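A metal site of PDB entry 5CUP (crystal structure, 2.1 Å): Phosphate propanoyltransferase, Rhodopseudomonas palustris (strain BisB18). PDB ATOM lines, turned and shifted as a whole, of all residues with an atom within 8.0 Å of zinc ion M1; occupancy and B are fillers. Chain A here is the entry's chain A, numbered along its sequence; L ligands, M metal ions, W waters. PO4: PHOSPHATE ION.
N of His 127 sits at hydrogen-bond distance from O of Glu 170. A ring nitrogen (NE2) of His 172 is in hydrogen-bond range of the side-chain carboxylate (OE1) of Glu 170 (3.1 Å). A ring nitrogen (ND1) of His 125 lies within hydrogen-bond range of the backbone carbonyl oxygen of Gln 123 (2.9 Å).
The nearest printed residue that does not touch zinc ion M1 is Arg 162 (5.5 Å).
Zinc ion M1 is bound by an oxygen (O3) of the ligand (2.0 Å). ND1 of His 172 binds zinc ion M1. A ring nitrogen (NE2) of His 127 binds zinc ion M1 (2.1 Å). Zinc ion M1 is bound by a ring nitrogen (NE2) of His 125, at 2.2 Å.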
ATOM      1  N   GLY A  11     -24.225  11.602   5.645  1.00  0.00           N
ATOM      2  CA  GLY A  11     -23.615  11.805   6.943  1.00  0.00           C
ATOM      3  C   GLY A  11     -23.840  13.246   7.368  1.00  0.00           C
ATOM      4  O   GLY A  11     -23.333  14.178   6.743  1.00  0.00           O
ATOM      5  N   SER A  13     -23.114  16.272   9.387  1.00  0.00           N
ATOM      6  CA  SER A  13     -21.973  16.801  10.119  1.00  0.00           C
ATOM      7  C   SER A  13     -22.364  17.949  11.047  1.00  0.00           C
ATOM      8  O   SER A  13     -22.666  19.050  10.603  1.00  0.00           O
ATOM      9  CB  SER A  13     -20.902  17.268   9.149  1.00  0.00           C
ATOM     10  OG  SER A  13     -20.120  18.306   9.714  1.00  0.00           O
ATOM     11  N   HIS A  16     -17.916  21.177  14.333  1.00  0.00           N
ATOM     12  CA  HIS A  16     -16.712  20.497  14.799  1.00  0.00           C
ATOM     13  C   HIS A  16     -15.449  21.258  14.437  1.00  0.00           C
ATOM     14  O   HIS A  16     -15.504  22.307  13.782  1.00  0.00           O
ATOM     15  CB  HIS A  16     -16.647  19.083  14.218  1.00  0.00           C
ATOM     16  CG  HIS A  16     -16.527  19.044  12.731  1.00  0.00           C
ATOM     17  ND1 HIS A  16     -17.613  18.894  11.888  1.00  0.00           N
ATOM     18  CD2 HIS A  16     -15.441  19.133  11.923  1.00  0.00           C
ATOM     19  CE1 HIS A  16     -17.196  18.897  10.640  1.00  0.00           C
ATOM     20  NE2 HIS A  16     -15.886  19.041  10.632  1.00  0.00           N
ATOM     21  N   HIS A  18     -11.051  20.815  13.429  1.00  0.00           N
ATOM     22  CA  HIS A  18      -9.806  20.091  13.162  1.00  0.00           C
ATOM     23  C   HIS A  18      -8.665  20.909  13.763  1.00  0.00           C
ATOM     24  O   HIS A  18      -8.662  22.129  13.654  1.00  0.00           O
ATOM     25  CB  HIS A  18      -9.607  19.881  11.668  1.00  0.00           C
ATOM     26  CG  HIS A  18     -10.795  19.298  10.965  1.00  0.00           C
ATOM     27  ND1 HIS A  18     -10.994  17.946  10.837  1.00  0.00           N
ATOM     28  CD2 HIS A  18     -11.859  19.901  10.376  1.00  0.00           C
ATOM     29  CE1 HIS A  18     -12.128  17.734  10.184  1.00  0.00           C
ATOM     30  NE2 HIS A  18     -12.667  18.895   9.891  1.00  0.00           N
ATOM     31  N   MET A  40     -15.531   7.155  12.201  1.00  0.00           N
ATOM     32  CA  MET A  40     -16.393   7.695  11.156  1.00  0.00           C
ATOM     33  C   MET A  40     -16.311   6.843   9.898  1.00  0.00           C
ATOM     34  O   MET A  40     -15.512   5.916   9.817  1.00  0.00           O
ATOM     35  CB  MET A  40     -15.997   9.150  10.845  1.00  0.00           C
ATOM     36  CG  MET A  40     -16.472  10.147  11.887  1.00  0.00           C
ATOM     37  SD  MET A  40     -15.618  11.730  11.803  1.00  0.00           S
ATOM     38  CE  MET A  40     -15.675  12.066  10.038  1.00  0.00           C
ATOM     39  N   GLN A  42     -15.472   7.863   6.746  1.00  0.00           N
ATOM     40  CA  GLN A  42     -14.222   8.146   6.050  1.00  0.00           C
ATOM     41  C   GLN A  42     -13.077   7.481   6.807  1.00  0.00           C
ATOM     42  O   GLN A  42     -12.903   7.728   7.997  1.00  0.00           O
ATOM     43  CB  GLN A  42     -13.983   9.653   5.934  1.00  0.00           C
ATOM     44  CG  GLN A  42     -15.077  10.390   5.173  1.00  0.00           C
ATOM     45  CD  GLN A  42     -15.301   9.838   3.778  1.00  0.00           C
ATOM     46  OE1 GLN A  42     -14.355   9.701   2.996  1.00  0.00           O
ATOM     47  NE2 GLN A  42     -16.539   9.489   3.460  1.00  0.00           N
ATOM     48  N   GLN A  45     -10.557   8.605   9.938  1.00  0.00           N
ATOM     49  CA  GLN A  45     -11.152   9.727  10.638  1.00  0.00           C
ATOM     50  C   GLN A  45     -12.100   9.249  11.732  1.00  0.00           C
ATOM     51  O   GLN A  45     -12.677   8.173  11.628  1.00  0.00           O
ATOM     52  CB  GLN A  45     -11.898  10.633   9.654  1.00  0.00           C
ATOM     53  CG  GLN A  45     -11.012  11.188   8.554  1.00  0.00           C
ATOM     54  CD  GLN A  45     -11.473  12.544   8.055  1.00  0.00           C
ATOM     55  OE1 GLN A  45     -11.630  13.482   8.830  1.00  0.00           O
ATOM     56  NE2 GLN A  45     -11.685  12.645   6.747  1.00  0.00           N
ATOM     57  N   LEU A  67     -12.467  16.446  15.758  1.00  0.00           N
ATOM     58  CA  LEU A  67     -12.310  15.295  14.880  1.00  0.00           C
ATOM     59  C   LEU A  67     -10.841  14.978  14.650  1.00  0.00           C
ATOM     60  O   LEU A  67     -10.042  15.870  14.354  1.00  0.00           O
ATOM     61  CB  LEU A  67     -12.996  15.548  13.529  1.00  0.00           C
ATOM     62  CG  LEU A  67     -14.509  15.763  13.520  1.00  0.00           C
ATOM     63  CD1 LEU A  67     -14.990  15.871  12.071  1.00  0.00           C
ATOM     64  CD2 LEU A  67     -15.246  14.647  14.232  1.00  0.00           C
ATOM     65  N   ARG A  71      -4.386  17.640  11.905  1.00  0.00           N
ATOM     66  CA  ARG A  71      -4.085  18.091  10.554  1.00  0.00           C
ATOM     67  C   ARG A  71      -2.985  19.148  10.566  1.00  0.00           C
ATOM     68  O   ARG A  71      -2.468  19.496  11.623  1.00  0.00           O
ATOM     69  CB  ARG A  71      -5.349  18.629   9.871  1.00  0.00           C
ATOM     70  CG  ARG A  71      -6.387  17.559   9.581  1.00  0.00           C
ATOM     71  CD  ARG A  71      -7.571  18.125   8.829  1.00  0.00           C
ATOM     72  NE  ARG A  71      -8.564  17.102   8.503  1.00  0.00           N
ATOM     73  CZ  ARG A  71      -9.740  17.335   7.938  1.00  0.00           C
ATOM     74  NH1 ARG A  71     -10.097  18.581   7.630  1.00  0.00           N
ATOM     75  NH2 ARG A  71     -10.566  16.330   7.689  1.00  0.00           N
ATOM     76  N   GLU A  77     -15.646  24.339  11.565  1.00  0.00           N
ATOM     77  CA  GLU A  77     -16.841  24.274  10.731  1.00  0.00           C
ATOM     78  C   GLU A  77     -18.092  24.479  11.567  1.00  0.00           C
ATOM     79  O   GLU A  77     -18.388  23.691  12.461  1.00  0.00           O
ATOM     80  CB  GLU A  77     -16.896  22.938   9.988  1.00  0.00           C
ATOM     81  CG  GLU A  77     -15.842  22.812   8.902  1.00  0.00           C
ATOM     82  CD  GLU A  77     -15.652  21.382   8.453  1.00  0.00           C
ATOM     83  OE1 GLU A  77     -14.519  20.876   8.568  1.00  0.00           O
ATOM     84  OE2 GLU A  77     -16.629  20.772   7.962  1.00  0.00           O
ATOM     85  N   SER A  95     -13.508  22.399   2.307  1.00  0.00           N
ATOM     86  CA  SER A  95     -12.428  22.134   3.249  1.00  0.00           C
ATOM     87  C   SER A  95     -11.068  22.588   2.706  1.00  0.00           C
ATOM     88  O   SER A  95     -10.727  22.310   1.558  1.00  0.00           O
ATOM     89  CB  SER A  95     -12.373  20.645   3.584  1.00  0.00           C
ATOM     90  OG  SER A  95     -12.756  20.404   4.923  1.00  0.00           O
ATOM     91  N   ALA A 122     -19.432  24.965   6.022  1.00  0.00           N
ATOM     92  CA  ALA A 122     -19.067  23.884   5.112  1.00  0.00           C
ATOM     93  C   ALA A 122     -19.976  23.844   3.890  1.00  0.00           C
ATOM     94  O   ALA A 122     -21.205  23.780   4.011  1.00  0.00           O
ATOM     95  CB  ALA A 122     -19.094  22.557   5.833  1.00  0.00           C
ATOM     96  N   GLN A 123     -19.365  23.886   2.703  1.00  0.00           N
ATOM     97  CA  GLN A 123     -20.095  23.626   1.470  1.00  0.00           C
ATOM     98  C   GLN A 123     -20.370  22.142   1.379  1.00  0.00           C
ATOM     99  O   GLN A 123     -19.472  21.329   1.563  1.00  0.00           O
ATOM    100  CB  GLN A 123     -19.292  24.108   0.249  1.00  0.00           C
ATOM    101  CG  GLN A 123     -19.991  23.863  -1.093  1.00  0.00           C
ATOM    102  CD  GLN A 123     -19.073  24.073  -2.277  1.00  0.00           C
ATOM    103  OE1 GLN A 123     -17.989  24.644  -2.155  1.00  0.00           O
ATOM    104  NE2 GLN A 123     -19.510  23.611  -3.450  1.00  0.00           N
ATOM    105  N   ARG A 124     -21.621  21.785   1.107  1.00  0.00           N
ATOM    106  CA  ARG A 124     -21.999  20.391   1.002  1.00  0.00           C
ATOM    107  C   ARG A 124     -21.185  19.713  -0.092  1.00  0.00           C
ATOM    108  O   ARG A 124     -20.818  20.339  -1.087  1.00  0.00           O
ATOM    109  CB  ARG A 124     -23.501  20.245   0.733  1.00  0.00           C
ATOM    110  CG  ARG A 124     -24.020  21.034  -0.457  1.00  0.00           C
ATOM    111  CD  ARG A 124     -25.522  20.896  -0.553  1.00  0.00           C
ATOM    112  NE  ARG A 124     -26.110  21.835  -1.511  1.00  0.00           N
ATOM    113  CZ  ARG A 124     -26.846  22.906  -1.199  1.00  0.00           C
ATOM    114  NH1 ARG A 124     -27.126  23.200   0.066  1.00  0.00           N
ATOM    115  NH2 ARG A 124     -27.316  23.682  -2.165  1.00  0.00           N
ATOM    116  N   HIS A 125     -20.898  18.430   0.110  1.00  0.00           N
ATOM    117  CA  HIS A 125     -19.984  17.710  -0.764  1.00  0.00           C
ATOM    118  C   HIS A 125     -20.171  16.205  -0.644  1.00  0.00           C
ATOM    119  O   HIS A 125     -20.833  15.723   0.284  1.00  0.00           O
ATOM    120  CB  HIS A 125     -18.540  18.084  -0.435  1.00  0.00           C
ATOM    121  CG  HIS A 125     -18.166  17.816   0.995  1.00  0.00           C
ATOM    122  ND1 HIS A 125     -18.402  18.720   2.014  1.00  0.00           N
ATOM    123  CD2 HIS A 125     -17.566  16.749   1.570  1.00  0.00           C
ATOM    124  CE1 HIS A 125     -17.970  18.222   3.153  1.00  0.00           C
ATOM    125  NE2 HIS A 125     -17.456  17.029   2.911  1.00  0.00           N
ATOM    126  N   ILE A 126     -19.593  15.479  -1.580  1.00  0.00           N
ATOM    127  CA  ILE A 126     -19.594  14.021  -1.557  1.00  0.00           C
ATOM    128  C   ILE A 126     -18.167  13.490  -1.614  1.00  0.00           C
ATOM    129  O   ILE A 126     -17.441  13.733  -2.573  1.00  0.00           O
ATOM    130  CB  ILE A 126     -20.408  13.425  -2.731  1.00  0.00           C
ATOM    131  CG1 ILE A 126     -21.867  13.899  -2.675  1.00  0.00           C
ATOM    132  CG2 ILE A 126     -20.349  11.896  -2.709  1.00  0.00           C
ATOM    133  CD1 ILE A 126     -22.695  13.492  -3.879  1.00  0.00           C
ATOM    134  N   HIS A 127     -17.773  12.774  -0.563  1.00  0.00           N
ATOM    135  CA  HIS A 127     -16.514  12.024  -0.583  1.00  0.00           C
ATOM    136  C   HIS A 127     -16.719  10.793  -1.436  1.00  0.00           C
ATOM    137  O   HIS A 127     -17.640  10.014  -1.199  1.00  0.00           O
ATOM    138  CB  HIS A 127     -16.093  11.633   0.833  1.00  0.00           C
ATOM    139  CG  HIS A 127     -15.857  12.787   1.749  1.00  0.00           C
ATOM    140  ND1 HIS A 127     -14.695  13.533   1.726  1.00  0.00           N
ATOM    141  CD2 HIS A 127     -16.621  13.316   2.730  1.00  0.00           C
ATOM    142  CE1 HIS A 127     -14.777  14.483   2.638  1.00  0.00           C
ATOM    143  NE2 HIS A 127     -15.925  14.371   3.272  1.00  0.00           N
ATOM    144  N   ARG A 162     -15.704  15.309  -4.198  1.00  0.00           N
ATOM    145  CA  ARG A 162     -14.371  15.187  -3.611  1.00  0.00           C
ATOM    146  C   ARG A 162     -13.852  13.764  -3.751  1.00  0.00           C
ATOM    147  O   ARG A 162     -14.291  12.852  -3.031  1.00  0.00           O
ATOM    148  CB  ARG A 162     -14.399  15.589  -2.137  1.00  0.00           C
ATOM    149  CG  ARG A 162     -13.962  17.018  -1.873  1.00  0.00           C
ATOM    150  CD  ARG A 162     -13.627  17.260  -0.407  1.00  0.00           C
ATOM    151  NE  ARG A 162     -12.634  16.309   0.089  1.00  0.00           N
ATOM    152  CZ  ARG A 162     -11.962  16.435   1.226  1.00  0.00           C
ATOM    153  NH1 ARG A 162     -12.157  17.487   2.008  1.00  0.00           N
ATOM    154  NH2 ARG A 162     -11.084  15.515   1.587  1.00  0.00           N
ATOM    155  N   GLU A 170     -19.877   8.855   0.506  1.00  0.00           N
ATOM    156  CA  GLU A 170     -20.702   9.469   1.538  1.00  0.00           C
ATOM    157  C   GLU A 170     -20.916  10.951   1.224  1.00  0.00           C
ATOM    158  O   GLU A 170     -20.005  11.611   0.714  1.00  0.00           O
ATOM    159  CB  GLU A 170     -20.052   9.303   2.913  1.00  0.00           C
ATOM    160  CG  GLU A 170     -20.836   9.918   4.067  1.00  0.00           C
ATOM    161  CD  GLU A 170     -20.073   9.897   5.382  1.00  0.00           C
ATOM    162  OE1 GLU A 170     -18.818   9.910   5.357  1.00  0.00           O
ATOM    163  OE2 GLU A 170     -20.725   9.861   6.452  1.00  0.00           O
ATOM    164  N   MET A 171     -22.104  11.454   1.539  1.00  0.00           N
ATOM    165  CA  MET A 171     -22.403  12.884   1.377  1.00  0.00           C
ATOM    166  C   MET A 171     -22.429  13.577   2.733  1.00  0.00           C
ATOM    167  O   MET A 171     -23.048  13.091   3.675  1.00  0.00           O
ATOM    168  CB  MET A 171     -23.737  13.075   0.665  1.00  0.00           C
ATOM    169  CG  MET A 171     -24.084  14.542   0.464  1.00  0.00           C
ATOM    170  SD  MET A 171     -25.503  14.799  -0.618  1.00  0.00           S
ATOM    171  CE  MET A 171     -25.446  16.581  -0.795  1.00  0.00           C
ATOM    172  N   HIS A 172     -21.742  14.716   2.816  1.00  0.00           N
ATOM    173  CA  HIS A 172     -21.678  15.508   4.042  1.00  0.00           C
ATOM    174  C   HIS A 172     -22.470  16.807   3.914  1.00  0.00           C
ATOM    175  O   HIS A 172     -22.217  17.608   3.011  1.00  0.00           O
ATOM    176  CB  HIS A 172     -20.227  15.810   4.415  1.00  0.00           C
ATOM    177  CG  HIS A 172     -19.527  14.672   5.097  1.00  0.00           C
ATOM    178  ND1 HIS A 172     -18.148  14.604   5.205  1.00  0.00           N
ATOM    179  CD2 HIS A 172     -20.004  13.578   5.731  1.00  0.00           C
ATOM    180  CE1 HIS A 172     -17.817  13.509   5.868  1.00  0.00           C
ATOM    181  NE2 HIS A 172     -18.923  12.867   6.194  1.00  0.00           N
ATOM    182  N   ILE A 173     -23.412  17.005   4.832  1.00  0.00           N
ATOM    183  CA  ILE A 173     -24.206  18.226   4.925  1.00  0.00           C
ATOM    184  C   ILE A 173     -24.285  18.641   6.392  1.00  0.00           C
ATOM    185  O   ILE A 173     -24.208  17.785   7.271  1.00  0.00           O
ATOM    186  CB  ILE A 173     -25.621  18.035   4.349  1.00  0.00           C
ATOM    187  CG1 ILE A 173     -26.320  16.860   5.048  1.00  0.00           C
ATOM    188  CG2 ILE A 173     -25.546  17.787   2.847  1.00  0.00           C
ATOM    189  CD1 ILE A 173     -27.786  16.719   4.700  1.00  0.00           C
HETATM  190  P   PO4 L   1     -14.243  17.350   6.384  1.00  0.00           P
HETATM  191  O1  PO4 L   1     -13.066  16.465   6.708  1.00  0.00           O
HETATM  192  O2  PO4 L   1     -15.087  17.547   7.619  1.00  0.00           O
HETATM  193  O3  PO4 L   1     -15.072  16.701   5.300  1.00  0.00           O
HETATM  194  O4  PO4 L   1     -13.750  18.682   5.884  1.00  0.00           O
HETATM  195 ZN    ZN M   1     -16.701  15.834   4.590  1.00  0.00          ZN
HETATM  196 ZN    ZN M   2     -14.571  18.957   9.008  1.00  0.00          ZN
HETATM  197  O   HOH W   1     -14.393  14.079   6.410  1.00  0.00           O
